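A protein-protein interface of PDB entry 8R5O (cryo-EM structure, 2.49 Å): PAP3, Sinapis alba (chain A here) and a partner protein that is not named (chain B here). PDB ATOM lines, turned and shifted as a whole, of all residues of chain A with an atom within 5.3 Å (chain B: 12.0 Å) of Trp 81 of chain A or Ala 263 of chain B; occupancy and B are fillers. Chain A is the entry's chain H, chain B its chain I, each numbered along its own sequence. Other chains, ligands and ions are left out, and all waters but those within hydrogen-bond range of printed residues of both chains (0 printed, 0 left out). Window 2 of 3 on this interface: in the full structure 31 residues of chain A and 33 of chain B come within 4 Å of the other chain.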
ATOM      1  N   ARG A  72     -18.874  20.815  19.963  1.00  0.00           N
ATOM      2  CA  ARG A  72     -19.284  22.154  19.556  1.00  0.00           C
ATOM      3  C   ARG A  72     -19.840  22.150  18.139  1.00  0.00           C
ATOM      4  O   ARG A  72     -20.859  22.793  17.862  1.00  0.00           O
ATOM      5  CB  ARG A  72     -18.106  23.119  19.679  1.00  0.00           C
ATOM      6  CG  ARG A  72     -18.264  24.407  18.898  1.00  0.00           C
ATOM      7  CD  ARG A  72     -17.313  25.479  19.398  1.00  0.00           C
ATOM      8  NE  ARG A  72     -16.034  24.924  19.823  1.00  0.00           N
ATOM      9  CZ  ARG A  72     -15.024  24.654  19.007  1.00  0.00           C
ATOM     10  NH1 ARG A  72     -15.113  24.864  17.704  1.00  0.00           N
ATOM     11  NH2 ARG A  72     -13.898  24.158  19.511  1.00  0.00           N
ATOM     12  N   ASN A  75     -23.261  20.503  18.316  1.00  0.00           N
ATOM     13  CA  ASN A  75     -24.298  21.396  18.823  1.00  0.00           C
ATOM     14  C   ASN A  75     -24.745  22.390  17.759  1.00  0.00           C
ATOM     15  O   ASN A  75     -25.931  22.725  17.677  1.00  0.00           O
ATOM     16  CB  ASN A  75     -23.804  22.126  20.070  1.00  0.00           C
ATOM     17  CG  ASN A  75     -23.873  21.262  21.310  1.00  0.00           C
ATOM     18  OD1 ASN A  75     -24.705  20.362  21.404  1.00  0.00           O
ATOM     19  ND2 ASN A  75     -23.000  21.532  22.269  1.00  0.00           N
ATOM     20  N   TRP A  76     -23.810  22.881  16.945  1.00  0.00           N
ATOM     21  CA  TRP A  76     -24.170  23.803  15.874  1.00  0.00           C
ATOM     22  C   TRP A  76     -25.047  23.118  14.832  1.00  0.00           C
ATOM     23  O   TRP A  76     -26.104  23.635  14.454  1.00  0.00           O
ATOM     24  CB  TRP A  76     -22.905  24.373  15.229  1.00  0.00           C
ATOM     25  CG  TRP A  76     -23.156  25.284  14.060  1.00  0.00           C
ATOM     26  CD1 TRP A  76     -23.477  24.915  12.785  1.00  0.00           C
ATOM     27  CD2 TRP A  76     -23.087  26.716  14.053  1.00  0.00           C
ATOM     28  NE1 TRP A  76     -23.623  26.025  11.993  1.00  0.00           N
ATOM     29  CE2 TRP A  76     -23.388  27.143  12.746  1.00  0.00           C
ATOM     30  CE3 TRP A  76     -22.802  27.677  15.028  1.00  0.00           C
ATOM     31  CZ2 TRP A  76     -23.414  28.489  12.388  1.00  0.00           C
ATOM     32  CZ3 TRP A  76     -22.830  29.010  14.671  1.00  0.00           C
ATOM     33  CH2 TRP A  76     -23.132  29.405  13.363  1.00  0.00           C
ATOM     34  N   ARG A  79     -28.167  20.697  16.956  1.00  0.00           N
ATOM     35  CA  ARG A  79     -29.007  21.362  17.940  1.00  0.00           C
ATOM     36  C   ARG A  79     -29.140  22.861  17.706  1.00  0.00           C
ATOM     37  O   ARG A  79     -29.781  23.543  18.511  1.00  0.00           O
ATOM     38  CB  ARG A  79     -28.467  21.100  19.350  1.00  0.00           C
ATOM     39  CG  ARG A  79     -27.953  19.684  19.549  1.00  0.00           C
ATOM     40  CD  ARG A  79     -27.765  19.355  21.016  1.00  0.00           C
ATOM     41  NE  ARG A  79     -28.992  18.849  21.617  1.00  0.00           N
ATOM     42  CZ  ARG A  79     -29.252  17.565  21.815  1.00  0.00           C
ATOM     43  NH1 ARG A  79     -28.379  16.625  21.492  1.00  0.00           N
ATOM     44  NH2 ARG A  79     -30.416  17.214  22.354  1.00  0.00           N
ATOM     45  N   GLY A  80     -28.559  23.389  16.634  1.00  0.00           N
ATOM     46  CA  GLY A  80     -28.716  24.794  16.309  1.00  0.00           C
ATOM     47  C   GLY A  80     -28.111  25.761  17.302  1.00  0.00           C
ATOM     48  O   GLY A  80     -28.656  26.849  17.500  1.00  0.00           O
ATOM     49  N   TRP A  81     -26.998  25.399  17.931  1.00  0.00           N
ATOM     50  CA  TRP A  81     -26.323  26.316  18.836  1.00  0.00           C
ATOM     51  C   TRP A  81     -25.624  27.426  18.061  1.00  0.00           C
ATOM     52  O   TRP A  81     -25.110  27.218  16.961  1.00  0.00           O
ATOM     53  CB  TRP A  81     -25.304  25.572  19.702  1.00  0.00           C
ATOM     54  CG  TRP A  81     -24.310  26.481  20.362  1.00  0.00           C
ATOM     55  CD1 TRP A  81     -24.475  27.168  21.526  1.00  0.00           C
ATOM     56  CD2 TRP A  81     -23.000  26.812  19.884  1.00  0.00           C
ATOM     57  NE1 TRP A  81     -23.350  27.903  21.808  1.00  0.00           N
ATOM     58  CE2 TRP A  81     -22.428  27.702  20.814  1.00  0.00           C
ATOM     59  CE3 TRP A  81     -22.255  26.440  18.762  1.00  0.00           C
ATOM     60  CZ2 TRP A  81     -21.148  28.224  20.656  1.00  0.00           C
ATOM     61  CZ3 TRP A  81     -20.984  26.959  18.607  1.00  0.00           C
ATOM     62  CH2 TRP A  81     -20.444  27.842  19.549  1.00  0.00           C
ATOM     63  N   ALA A  82     -25.615  28.620  18.648  1.00  0.00           N
ATOM     64  CA  ALA A  82     -24.832  29.736  18.144  1.00  0.00           C
ATOM     65  C   ALA A  82     -24.451  30.615  19.322  1.00  0.00           C
ATOM     66  O   ALA A  82     -25.252  30.783  20.249  1.00  0.00           O
ATOM     67  CB  ALA A  82     -25.602  30.554  17.098  1.00  0.00           C
ATOM     68  N   PRO A  83     -23.248  31.182  19.322  1.00  0.00           N
ATOM     69  CA  PRO A  83     -22.833  32.074  20.425  1.00  0.00           C
ATOM     70  C   PRO A  83     -23.410  33.477  20.278  1.00  0.00           C
ATOM     71  O   PRO A  83     -22.712  34.457  20.009  1.00  0.00           O
ATOM     72  CB  PRO A  83     -21.306  32.043  20.310  1.00  0.00           C
ATOM     73  CG  PRO A  83     -21.056  31.840  18.861  1.00  0.00           C
ATOM     74  CD  PRO A  83     -22.153  30.938  18.367  1.00  0.00           C
ATOM     75  N   ASN A 308     -29.324  28.853  12.935  1.00  0.00           N
ATOM     76  CA  ASN A 308     -27.915  29.229  12.995  1.00  0.00           C
ATOM     77  C   ASN A 308     -27.486  30.071  11.805  1.00  0.00           C
ATOM     78  O   ASN A 308     -26.547  30.865  11.921  1.00  0.00           O
ATOM     79  CB  ASN A 308     -27.039  27.979  13.075  1.00  0.00           C
ATOM     80  CG  ASN A 308     -26.937  27.434  14.471  1.00  0.00           C
ATOM     81  OD1 ASN A 308     -26.488  26.311  14.675  1.00  0.00           O
ATOM     82  ND2 ASN A 308     -27.359  28.226  15.449  1.00  0.00           N
ATOM     83  N   PRO B 258     -20.426  24.261   7.076  1.00  0.00           N
ATOM     84  CA  PRO B 258     -20.576  25.553   7.752  1.00  0.00           C
ATOM     85  C   PRO B 258     -19.299  25.991   8.452  1.00  0.00           C
ATOM     86  O   PRO B 258     -18.475  25.176   8.871  1.00  0.00           O
ATOM     87  CB  PRO B 258     -21.700  25.296   8.761  1.00  0.00           C
ATOM     88  CG  PRO B 258     -21.635  23.835   9.022  1.00  0.00           C
ATOM     89  CD  PRO B 258     -21.215  23.200   7.728  1.00  0.00           C
ATOM     90  N   THR B 259     -19.146  27.309   8.572  1.00  0.00           N
ATOM     91  CA  THR B 259     -18.050  27.906   9.327  1.00  0.00           C
ATOM     92  C   THR B 259     -18.507  28.072  10.772  1.00  0.00           C
ATOM     93  O   THR B 259     -19.421  28.853  11.056  1.00  0.00           O
ATOM     94  CB  THR B 259     -17.639  29.245   8.723  1.00  0.00           C
ATOM     95  OG1 THR B 259     -17.199  29.045   7.373  1.00  0.00           O
ATOM     96  CG2 THR B 259     -16.513  29.872   9.528  1.00  0.00           C
ATOM     97  N   ILE B 260     -17.875  27.346  11.681  1.00  0.00           N
ATOM     98  CA  ILE B 260     -18.317  27.249  13.069  1.00  0.00           C
ATOM     99  C   ILE B 260     -17.332  28.021  13.941  1.00  0.00           C
ATOM    100  O   ILE B 260     -16.136  27.704  13.939  1.00  0.00           O
ATOM    101  CB  ILE B 260     -18.433  25.787  13.521  1.00  0.00           C
ATOM    102  CG1 ILE B 260     -19.350  25.024  12.564  1.00  0.00           C
ATOM    103  CG2 ILE B 260     -18.959  25.711  14.944  1.00  0.00           C
ATOM    104  CD1 ILE B 260     -19.498  23.570  12.893  1.00  0.00           C
ATOM    105  N   PRO B 261     -17.779  29.031  14.682  1.00  0.00           N
ATOM    106  CA  PRO B 261     -16.857  29.793  15.528  1.00  0.00           C
ATOM    107  C   PRO B 261     -16.295  28.946  16.658  1.00  0.00           C
ATOM    108  O   PRO B 261     -16.949  28.038  17.174  1.00  0.00           O
ATOM    109  CB  PRO B 261     -17.726  30.931  16.075  1.00  0.00           C
ATOM    110  CG  PRO B 261     -18.949  30.947  15.222  1.00  0.00           C
ATOM    111  CD  PRO B 261     -19.154  29.545  14.763  1.00  0.00           C
ATOM    112  N   ILE B 262     -15.056  29.263  17.044  1.00  0.00           N
ATOM    113  CA  ILE B 262     -14.429  28.594  18.182  1.00  0.00           C
ATOM    114  C   ILE B 262     -14.909  29.155  19.509  1.00  0.00           C
ATOM    115  O   ILE B 262     -14.669  28.540  20.556  1.00  0.00           O
ATOM    116  CB  ILE B 262     -12.895  28.694  18.069  1.00  0.00           C
ATOM    117  CG1 ILE B 262     -12.453  28.444  16.627  1.00  0.00           C
ATOM    118  CG2 ILE B 262     -12.214  27.682  18.978  1.00  0.00           C
ATOM    119  CD1 ILE B 262     -12.784  27.056  16.115  1.00  0.00           C
ATOM    120  N   ALA B 263     -15.595  30.294  19.497  1.00  0.00           N
ATOM    121  CA  ALA B 263     -16.130  30.892  20.713  1.00  0.00           C
ATOM    122  C   ALA B 263     -17.169  29.983  21.360  1.00  0.00           C
ATOM    123  O   ALA B 263     -18.178  30.451  21.882  1.00  0.00           O
ATOM    124  CB  ALA B 263     -16.735  32.254  20.408  1.00  0.00           C
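Of chain B, only Pro 261 and Ile 262 come within 4 Å of Arg 72 of chain A. Asn 75 of chain A touches none of the printed residues of chain B. Of chain B, only Pro 258 and Pro 261 come within 4 Å of Trp 76 of chain A. No residue of chain B comes within 4 Å of Gly 80 of chain A. Trp 81 of chain A touches just one residue of chain B: Ala 263 (3.9 Å). No residue of chain B comes within 4 Å of Ala 82 of chain A. Of chain B, only Ala 263 comes within 4 Å of Pro 83 of chain A. No residue of chain B comes within 4 Å of Asn 308 of chain A. Of the printed residues of chain A, Pro 258 of chain B touches Trp 76 (3.8 Å). Thr 259 of chain B touches none of the printed residues of chain A. Of the printed residues of chain A, Pro 261 of chain B touches Arg 72 (3.4 Å) and Trp 76 (3.7 Å). Of the printed residues of chain A, Ile 262 of chain B touches Arg 72 (3.6 Å). Ala 263 of chain B touches just these residues of chain A: Trp 81 (3.9 Å) and Pro 83 (3.8 Å). The nearest residue of chain B that does not touch Trp 81 of chain A is Pro 261 of chain B (4.2 Å). The nearest residue of chain A that does not touch Ala 263 of chain B is Arg 72 of chain A (4.9 Å).
Arg 72 of chain A touches Pro 261 of chain B. Arg 72 of chain A touches Ile 262 of chain B. CB of Pro 258 of chain B touches NE1 of Trp 76 of chain A (3.8 Å). CD of Pro 261 of chain B touches CZ3 of Trp 76 of chain A (3.7 Å). O of Ala 263 of chain B touches CZ2 of Trp 81 of chain A (3.9 Å). Pro 83 of chain A touches Ala 263 of chain B (CB to O, 3.8 Å).
The backbone carbonyl oxygen of Asn 75 of chain A is in hydrogen-bond range of the backbone NH of Trp 81 of chain A (2.9 Å). O of Trp 76 of chain A lies close to OD1 of Asn 308 of chain A, 2.7 Å away. O of Trp 81 of chain A lies close to OD1 of Asn 308 of chain A (2.8 Å).
Of the 6 printed residues of chain B, 4 touch a printed residue of chain A. Printed residues of chain B that touch a printed residue of chain A: Pro 258, Pro 261, Ile 262 and Ala 263. Hydrophobic or aromatic side chains of chain B within 4 Å of the printed part of chain A: Pro 258, Pro 261 and Ile 262. Hydrophobic or aromatic side chains of chain A that line the printed part of chain B: Trp 76, Trp 81 and Pro 83. Along chain A the printed residues that touch a printed residue of chain B span positions 72 to 83. Among the printed residues, no Asp or Glu carboxylate lies within 4 Å of a Lys or Arg side-chain nitrogen of the other chain.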
